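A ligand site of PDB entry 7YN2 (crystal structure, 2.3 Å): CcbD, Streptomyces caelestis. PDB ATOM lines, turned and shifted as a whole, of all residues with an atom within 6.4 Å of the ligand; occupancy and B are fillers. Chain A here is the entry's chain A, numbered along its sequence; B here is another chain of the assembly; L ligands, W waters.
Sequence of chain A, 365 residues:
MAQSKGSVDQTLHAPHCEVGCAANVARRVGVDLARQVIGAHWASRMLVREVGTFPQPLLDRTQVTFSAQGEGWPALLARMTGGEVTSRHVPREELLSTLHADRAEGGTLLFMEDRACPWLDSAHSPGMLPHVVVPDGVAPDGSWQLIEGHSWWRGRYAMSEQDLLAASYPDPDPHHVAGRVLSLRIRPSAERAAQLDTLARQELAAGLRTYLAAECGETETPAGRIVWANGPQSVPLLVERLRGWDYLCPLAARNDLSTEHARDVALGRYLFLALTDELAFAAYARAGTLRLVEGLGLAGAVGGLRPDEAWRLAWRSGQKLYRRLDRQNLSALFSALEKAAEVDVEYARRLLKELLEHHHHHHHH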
ATOM      1  N   CYS A  17      -9.486  11.683  24.357  1.00  0.00           N
ATOM      2  CA  CYS A  17     -10.691  11.512  25.163  1.00  0.00           C
ATOM      3  C   CYS A  17     -11.054  12.785  25.912  1.00  0.00           C
ATOM      4  O   CYS A  17     -12.230  13.084  26.084  1.00  0.00           O
ATOM      5  CB  CYS A  17     -10.549  10.320  26.126  1.00  0.00           C
ATOM      6  SG  CYS A  17      -9.227  10.386  27.326  1.00  0.00           S
ATOM      7  N   MET A 112      -9.336  10.293  36.708  1.00  0.00           N
ATOM      8  CA  MET A 112      -9.144   9.051  37.458  1.00  0.00           C
ATOM      9  C   MET A 112      -8.154   8.162  36.733  1.00  0.00           C
ATOM     10  O   MET A 112      -7.822   8.366  35.568  1.00  0.00           O
ATOM     11  CB  MET A 112     -10.455   8.275  37.668  1.00  0.00           C
ATOM     12  CG  MET A 112     -11.645   9.065  38.196  1.00  0.00           C
ATOM     13  SD  MET A 112     -13.166   8.657  37.326  1.00  0.00           S
ATOM     14  CE  MET A 112     -13.240   6.891  37.558  1.00  0.00           C
ATOM     15  N   ASP A 114      -6.934   4.496  35.062  1.00  0.00           N
ATOM     16  CA  ASP A 114      -7.606   3.558  34.157  1.00  0.00           C
ATOM     17  C   ASP A 114      -8.245   2.405  34.929  1.00  0.00           C
ATOM     18  O   ASP A 114      -9.284   1.880  34.505  1.00  0.00           O
ATOM     19  CB  ASP A 114      -6.609   2.975  33.161  1.00  0.00           C
ATOM     20  CG  ASP A 114      -6.238   3.937  32.052  1.00  0.00           C
ATOM     21  OD1 ASP A 114      -6.592   5.133  32.100  1.00  0.00           O
ATOM     22  OD2 ASP A 114      -5.573   3.475  31.103  1.00  0.00           O
ATOM     23  N   LEU A 120     -12.721   0.244  30.957  1.00  0.00           N
ATOM     24  CA  LEU A 120     -11.415   0.321  30.310  1.00  0.00           C
ATOM     25  C   LEU A 120     -10.674  -1.010  30.366  1.00  0.00           C
ATOM     26  O   LEU A 120      -9.724  -1.210  29.601  1.00  0.00           O
ATOM     27  CB  LEU A 120     -10.589   1.423  30.966  1.00  0.00           C
ATOM     28  CG  LEU A 120     -11.017   2.863  30.629  1.00  0.00           C
ATOM     29  CD1 LEU A 120      -9.931   3.879  30.951  1.00  0.00           C
ATOM     30  CD2 LEU A 120     -11.390   2.975  29.176  1.00  0.00           C
ATOM     31  N   SER A 122      -8.706  -2.231  32.675  1.00  0.00           N
ATOM     32  CA  SER A 122      -7.321  -1.932  33.012  1.00  0.00           C
ATOM     33  C   SER A 122      -7.084  -2.135  34.497  1.00  0.00           C
ATOM     34  O   SER A 122      -6.473  -1.283  35.161  1.00  0.00           O
ATOM     35  CB  SER A 122      -6.975  -0.506  32.578  1.00  0.00           C
ATOM     36  OG  SER A 122      -5.574  -0.320  32.458  1.00  0.00           O
ATOM     37  N   SER A 125      -3.247  -2.160  36.002  1.00  0.00           N
ATOM     38  CA  SER A 125      -2.327  -1.069  35.698  1.00  0.00           C
ATOM     39  C   SER A 125      -3.033   0.273  35.663  1.00  0.00           C
ATOM     40  O   SER A 125      -4.104   0.384  35.045  1.00  0.00           O
ATOM     41  CB  SER A 125      -1.638  -1.292  34.350  1.00  0.00           C
ATOM     42  OG  SER A 125      -1.379  -0.042  33.732  1.00  0.00           O
ATOM     43  N   PRO A 126      -2.470   1.312  36.273  1.00  0.00           N
ATOM     44  CA  PRO A 126      -3.078   2.650  36.224  1.00  0.00           C
ATOM     45  C   PRO A 126      -2.826   3.406  34.922  1.00  0.00           C
ATOM     46  O   PRO A 126      -3.218   4.580  34.826  1.00  0.00           O
ATOM     47  CB  PRO A 126      -2.403   3.379  37.394  1.00  0.00           C
ATOM     48  CG  PRO A 126      -1.065   2.741  37.492  1.00  0.00           C
ATOM     49  CD  PRO A 126      -1.206   1.300  37.034  1.00  0.00           C
ATOM     50  N   GLY A 127      -2.178   2.783  33.940  1.00  0.00           N
ATOM     51  CA  GLY A 127      -1.957   3.408  32.657  1.00  0.00           C
ATOM     52  C   GLY A 127      -0.734   4.317  32.613  1.00  0.00           C
ATOM     53  O   GLY A 127      -0.183   4.735  33.631  1.00  0.00           O
ATOM     54  N   MET A 128      -0.329   4.630  31.387  1.00  0.00           N
ATOM     55  CA  MET A 128       0.778   5.554  31.177  1.00  0.00           C
ATOM     56  C   MET A 128       0.417   6.968  31.619  1.00  0.00           C
ATOM     57  O   MET A 128       1.180   7.619  32.330  1.00  0.00           O
ATOM     58  CB  MET A 128       1.183   5.529  29.708  1.00  0.00           C
ATOM     59  CG  MET A 128       1.506   4.136  29.235  1.00  0.00           C
ATOM     60  SD  MET A 128       3.265   3.853  29.444  1.00  0.00           S
ATOM     61  CE  MET A 128       3.337   3.290  31.148  1.00  0.00           C
ATOM     62  N   LEU A 129      -0.749   7.448  31.192  1.00  0.00           N
ATOM     63  CA  LEU A 129      -1.326   8.714  31.614  1.00  0.00           C
ATOM     64  C   LEU A 129      -2.649   8.470  32.334  1.00  0.00           C
ATOM     65  O   LEU A 129      -3.261   7.402  32.181  1.00  0.00           O
ATOM     66  CB  LEU A 129      -1.561   9.629  30.401  1.00  0.00           C
ATOM     67  CG  LEU A 129      -0.340   9.868  29.507  1.00  0.00           C
ATOM     68  CD1 LEU A 129      -0.773  10.166  28.086  1.00  0.00           C
ATOM     69  CD2 LEU A 129       0.453  11.012  30.082  1.00  0.00           C
ATOM     70  N   PRO A 130      -3.124   9.414  33.140  1.00  0.00           N
ATOM     71  CA  PRO A 130      -4.445   9.260  33.739  1.00  0.00           C
ATOM     72  C   PRO A 130      -5.542   9.407  32.701  1.00  0.00           C
ATOM     73  O   PRO A 130      -5.322   9.875  31.570  1.00  0.00           O
ATOM     74  CB  PRO A 130      -4.503  10.398  34.772  1.00  0.00           C
ATOM     75  CG  PRO A 130      -3.600  11.425  34.232  1.00  0.00           C
ATOM     76  CD  PRO A 130      -2.483  10.675  33.568  1.00  0.00           C
ATOM     77  N   HIS A 131      -6.738   8.995  33.091  1.00  0.00           N
ATOM     78  CA  HIS A 131      -7.942   9.085  32.269  1.00  0.00           C
ATOM     79  C   HIS A 131      -8.792  10.260  32.723  1.00  0.00           C
ATOM     80  O   HIS A 131      -8.487  10.942  33.709  1.00  0.00           O
ATOM     81  CB  HIS A 131      -8.733   7.779  32.338  1.00  0.00           C
ATOM     82  CG  HIS A 131      -9.786   7.662  31.286  1.00  0.00           C
ATOM     83  ND1 HIS A 131      -9.518   7.854  29.958  1.00  0.00           N
ATOM     84  CD2 HIS A 131     -11.102   7.364  31.379  1.00  0.00           C
ATOM     85  CE1 HIS A 131     -10.634   7.684  29.256  1.00  0.00           C
ATOM     86  NE2 HIS A 131     -11.605   7.393  30.097  1.00  0.00           N
ATOM     87  N   VAL A 132      -9.865  10.507  31.978  1.00  0.00           N
ATOM     88  CA  VAL A 132     -10.778  11.608  32.283  1.00  0.00           C
ATOM     89  C   VAL A 132     -12.204  11.182  31.919  1.00  0.00           C
ATOM     90  O   VAL A 132     -12.406  10.465  30.927  1.00  0.00           O
ATOM     91  CB  VAL A 132     -10.366  12.890  31.550  1.00  0.00           C
ATOM     92  CG1 VAL A 132     -10.329  12.654  30.042  1.00  0.00           C
ATOM     93  CG2 VAL A 132     -11.260  14.058  31.936  1.00  0.00           C
ATOM     94  N   HIS A 150     -13.798   8.933  24.978  1.00  0.00           N
ATOM     95  CA  HIS A 150     -12.932   8.277  24.006  1.00  0.00           C
ATOM     96  C   HIS A 150     -13.740   7.456  23.011  1.00  0.00           C
ATOM     97  O   HIS A 150     -14.523   6.598  23.410  1.00  0.00           O
ATOM     98  CB  HIS A 150     -11.910   7.378  24.711  1.00  0.00           C
ATOM     99  CG  HIS A 150     -10.703   7.081  23.874  1.00  0.00           C
ATOM    100  ND1 HIS A 150     -10.770   6.890  22.506  1.00  0.00           N
ATOM    101  CD2 HIS A 150      -9.389   6.982  24.204  1.00  0.00           C
ATOM    102  CE1 HIS A 150      -9.554   6.674  22.031  1.00  0.00           C
ATOM    103  NE2 HIS A 150      -8.700   6.723  23.045  1.00  0.00           N
ATOM    104  N   TRP A 152     -13.153   4.878  21.428  1.00  0.00           N
ATOM    105  CA  TRP A 152     -13.123   3.429  21.594  1.00  0.00           C
ATOM    106  C   TRP A 152     -14.127   2.949  22.644  1.00  0.00           C
ATOM    107  O   TRP A 152     -14.549   1.786  22.590  1.00  0.00           O
ATOM    108  CB  TRP A 152     -11.721   2.959  21.961  1.00  0.00           C
ATOM    109  CG  TRP A 152     -11.382   1.525  21.559  1.00  0.00           C
ATOM    110  CD1 TRP A 152     -10.758   0.591  22.329  1.00  0.00           C
ATOM    111  CD2 TRP A 152     -11.639   0.877  20.292  1.00  0.00           C
ATOM    112  NE1 TRP A 152     -10.611  -0.594  21.638  1.00  0.00           N
ATOM    113  CE2 TRP A 152     -11.140  -0.441  20.379  1.00  0.00           C
ATOM    114  CE3 TRP A 152     -12.244   1.290  19.086  1.00  0.00           C
ATOM    115  CZ2 TRP A 152     -11.224  -1.355  19.327  1.00  0.00           C
ATOM    116  CZ3 TRP A 152     -12.319   0.376  18.039  1.00  0.00           C
ATOM    117  CH2 TRP A 152     -11.820  -0.932  18.170  1.00  0.00           C
ATOM    118  N   TRP A 153     -14.520   3.804  23.584  1.00  0.00           N
ATOM    119  CA  TRP A 153     -15.445   3.421  24.647  1.00  0.00           C
ATOM    120  C   TRP A 153     -16.599   4.404  24.811  1.00  0.00           C
ATOM    121  O   TRP A 153     -17.278   4.367  25.844  1.00  0.00           O
ATOM    122  CB  TRP A 153     -14.707   3.282  25.983  1.00  0.00           C
ATOM    123  CG  TRP A 153     -13.705   2.170  26.048  1.00  0.00           C
ATOM    124  CD1 TRP A 153     -13.955   0.841  26.247  1.00  0.00           C
ATOM    125  CD2 TRP A 153     -12.290   2.297  25.934  1.00  0.00           C
ATOM    126  NE1 TRP A 153     -12.782   0.135  26.259  1.00  0.00           N
ATOM    127  CE2 TRP A 153     -11.737   0.998  26.072  1.00  0.00           C
ATOM    128  CE3 TRP A 153     -11.425   3.377  25.713  1.00  0.00           C
ATOM    129  CZ2 TRP A 153     -10.373   0.757  26.004  1.00  0.00           C
ATOM    130  CZ3 TRP A 153     -10.067   3.132  25.656  1.00  0.00           C
ATOM    131  CH2 TRP A 153      -9.551   1.837  25.800  1.00  0.00           C
ATOM    132  N   HIS A 175      -0.292   9.248  39.226  1.00  0.00           N
ATOM    133  CA  HIS A 175      -0.562  10.289  38.249  1.00  0.00           C
ATOM    134  C   HIS A 175      -0.815  11.658  38.887  1.00  0.00           C
ATOM    135  O   HIS A 175      -1.081  12.606  38.150  1.00  0.00           O
ATOM    136  CB  HIS A 175      -1.744   9.886  37.358  1.00  0.00           C
ATOM    137  CG  HIS A 175      -1.477   8.698  36.483  1.00  0.00           C
ATOM    138  ND1 HIS A 175      -0.308   8.552  35.762  1.00  0.00           N
ATOM    139  CD2 HIS A 175      -2.220   7.603  36.208  1.00  0.00           C
ATOM    140  CE1 HIS A 175      -0.357   7.416  35.087  1.00  0.00           C
ATOM    141  NE2 HIS A 175      -1.507   6.816  35.337  1.00  0.00           N
ATOM    142  N   TYR A 270       5.543   2.813  20.682  1.00  0.00           N
ATOM    143  CA  TYR A 270       4.741   3.789  21.427  1.00  0.00           C
ATOM    144  C   TYR A 270       4.838   5.188  20.816  1.00  0.00           C
ATOM    145  O   TYR A 270       3.848   5.928  20.804  1.00  0.00           O
ATOM    146  CB  TYR A 270       5.182   3.815  22.900  1.00  0.00           C
ATOM    147  CG  TYR A 270       4.211   4.564  23.827  1.00  0.00           C
ATOM    148  CD1 TYR A 270       2.843   4.511  23.622  1.00  0.00           C
ATOM    149  CD2 TYR A 270       4.683   5.323  24.894  1.00  0.00           C
ATOM    150  CE1 TYR A 270       1.953   5.196  24.449  1.00  0.00           C
ATOM    151  CE2 TYR A 270       3.785   6.018  25.736  1.00  0.00           C
ATOM    152  CZ  TYR A 270       2.429   5.949  25.508  1.00  0.00           C
ATOM    153  OH  TYR A 270       1.527   6.640  26.338  1.00  0.00           O
ATOM    154  N   LEU A 273       2.372   5.063  18.074  1.00  0.00           N
ATOM    155  CA  LEU A 273       0.979   5.110  18.560  1.00  0.00           C
ATOM    156  C   LEU A 273       0.568   6.539  18.905  1.00  0.00           C
ATOM    157  O   LEU A 273      -0.472   7.024  18.432  1.00  0.00           O
ATOM    158  CB  LEU A 273       0.787   4.207  19.768  1.00  0.00           C
ATOM    159  CG  LEU A 273      -0.702   4.136  20.183  1.00  0.00           C
ATOM    160  CD1 LEU A 273      -1.532   3.308  19.208  1.00  0.00           C
ATOM    161  CD2 LEU A 273      -0.863   3.580  21.578  1.00  0.00           C
ATOM    162  N   ASP B  60       4.012  11.910  27.172  1.00  0.00           N
ATOM    163  CA  ASP B  60       3.718  10.539  26.801  1.00  0.00           C
ATOM    164  C   ASP B  60       3.352   9.641  27.974  1.00  0.00           C
ATOM    165  O   ASP B  60       2.707   8.602  27.761  1.00  0.00           O
ATOM    166  CB  ASP B  60       4.922   9.940  26.055  1.00  0.00           C
ATOM    167  CG  ASP B  60       6.208   9.955  26.886  1.00  0.00           C
ATOM    168  OD1 ASP B  60       6.551  10.974  27.545  1.00  0.00           O
ATOM    169  OD2 ASP B  60       6.896   8.918  26.869  1.00  0.00           O
ATOM    170  N   GLU B 260       0.301  -3.532  25.110  1.00  0.00           N
ATOM    171  CA  GLU B 260       0.211  -2.269  25.855  1.00  0.00           C
ATOM    172  C   GLU B 260       0.612  -2.447  27.312  1.00  0.00           C
ATOM    173  O   GLU B 260       1.339  -1.608  27.860  1.00  0.00           O
ATOM    174  CB  GLU B 260      -1.211  -1.695  25.758  1.00  0.00           C
ATOM    175  CG  GLU B 260      -1.646  -1.307  24.354  1.00  0.00           C
ATOM    176  CD  GLU B 260      -1.869  -2.515  23.438  1.00  0.00           C
ATOM    177  OE1 GLU B 260      -2.196  -3.609  23.949  1.00  0.00           O
ATOM    178  OE2 GLU B 260      -1.704  -2.364  22.216  1.00  0.00           O
ATOM    179  N   ARG B 263       4.253  -2.921  27.309  1.00  0.00           N
ATOM    180  CA  ARG B 263       4.894  -1.630  27.179  1.00  0.00           C
ATOM    181  C   ARG B 263       4.947  -0.898  28.526  1.00  0.00           C
ATOM    182  O   ARG B 263       5.930  -0.223  28.840  1.00  0.00           O
ATOM    183  CB  ARG B 263       4.177  -0.794  26.121  1.00  0.00           C
ATOM    184  CG  ARG B 263       4.623   0.645  25.995  1.00  0.00           C
ATOM    185  CD  ARG B 263       3.475   1.527  25.549  1.00  0.00           C
ATOM    186  NE  ARG B 263       2.366   1.471  26.493  1.00  0.00           N
ATOM    187  CZ  ARG B 263       1.082   1.578  26.173  1.00  0.00           C
ATOM    188  NH1 ARG B 263       0.687   1.773  24.925  1.00  0.00           N
ATOM    189  NH2 ARG B 263       0.173   1.491  27.142  1.00  0.00           N
ATOM    190  N   ASP B 264       3.895  -1.056  29.345  1.00  0.00           N
ATOM    191  CA  ASP B 264       3.897  -0.465  30.681  1.00  0.00           C
ATOM    192  C   ASP B 264       5.004  -1.057  31.549  1.00  0.00           C
ATOM    193  O   ASP B 264       5.641  -0.339  32.337  1.00  0.00           O
ATOM    194  CB  ASP B 264       2.544  -0.689  31.374  1.00  0.00           C
ATOM    195  CG  ASP B 264       1.404   0.055  30.699  1.00  0.00           C
ATOM    196  OD1 ASP B 264       1.600   0.679  29.636  1.00  0.00           O
ATOM    197  OD2 ASP B 264       0.278   0.009  31.245  1.00  0.00           O
HETATM  198  C1  LIG L   1      -3.507   4.569  29.151  1.00  0.00           C
HETATM  199  C2  LIG L   1      -2.827   3.327  28.493  1.00  0.00           C
HETATM  200  C3  LIG L   1      -2.668   3.492  26.938  1.00  0.00           C
HETATM  201  C4  LIG L   1      -4.038   3.867  26.302  1.00  0.00           C
HETATM  202  C5  LIG L   1      -4.871   4.795  28.332  1.00  0.00           C
HETATM  203  C6  LIG L   1      -5.964   5.753  28.938  1.00  0.00           C
HETATM  204  C7  LIG L   1      -5.529   7.211  28.987  1.00  0.00           C
HETATM  205  C8  LIG L   1      -6.714   8.130  28.639  1.00  0.00           C
HETATM  206  C9  LIG L   1      -5.037   1.688  24.914  1.00  0.00           C
HETATM  207  N1  LIG L   1      -7.276   5.681  28.234  1.00  0.00           N
HETATM  208  O1  LIG L   1      -4.562   5.107  26.920  1.00  0.00           O
HETATM  209  O2  LIG L   1      -2.151   2.261  26.311  1.00  0.00           O
HETATM  210  O3  LIG L   1      -2.568   5.726  29.210  1.00  0.00           O
HETATM  211  O4  LIG L   1      -1.581   2.981  29.153  1.00  0.00           O
HETATM  212  O5  LIG L   1      -5.057   7.478  30.307  1.00  0.00           O
HETATM  213  S1  LIG L   1      -5.402   2.675  26.359  1.00  0.00           S
HETATM  214  O   HOH W   1      -0.958   6.487  26.935  1.00  0.00           O
HETATM  215  O   HOH W   2      -1.901   0.596  30.089  1.00  0.00           O
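Water W2 lies within hydrogen-bond range of OD2 of Asp 264 of chain B (2.5 Å) and O4 of the ligand (2.6 Å). Water W1 lies within hydrogen-bond range of the side-chain hydroxyl (OH) of Tyr 270 (2.6 Å) and an oxygen (O3) of the ligand (2.9 Å).
An oxygen (O2) of the ligand is in hydrogen-bond range of the guanidinium group (NH2) of Arg 263 of chain B (2.6 Å). The backbone NH (N) of Leu 129 sits at hydrogen-bond distance from an oxygen (O3) of the ligand. O5 of the ligand lies within hydrogen-bond range of O of Leu 129, at 2.6 Å. O of Pro 130 sits at hydrogen-bond distance from O5 of the ligand. The side-chain carboxylate (OD1) of Asp 114 lies within salt-bridge range of a nitrogen (N1) of the ligand, at 3.96 Å. The backbone NH (N) of Met 128 lies within hydrogen-bond range of an oxygen (O4) of the ligand (3.0 Å).
NH2 of Arg 263 of chain B is in salt-bridge range of OD1 of Asp 264 of chain B. NH2 of Arg 263 of chain B lies within hydrogen-bond range of O of Glu 260 of chain B (3.4 Å). ND1 of His 131 lies close to SG of Cys 17, at 3.7 Å. N of His 131 lies within hydrogen-bond range of O of Met 112 (2.8 Å). The side-chain hydroxyl of Ser 125 sits at hydrogen-bond distance from the backbone NH of Gly 127, at 2.9 Å. The backbone carbonyl oxygen of Gly 127 is in hydrogen-bond range of a ring nitrogen (NE2) of His 175, at 3.0 Å. OD2 of Asp 264 of chain B is in hydrogen-bond range of OG of Ser 125, at 3.0 Å.
Merely in contact with the ligand: His 131 (3.1 Å), Gly 127 (3.5 Å), Cys 17 (3.6 Å) and Asp 264 of chain B (3.96 Å). Hydrophobic or aromatic side chains within 4 Å of the ligand: Met 128 and His 131.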
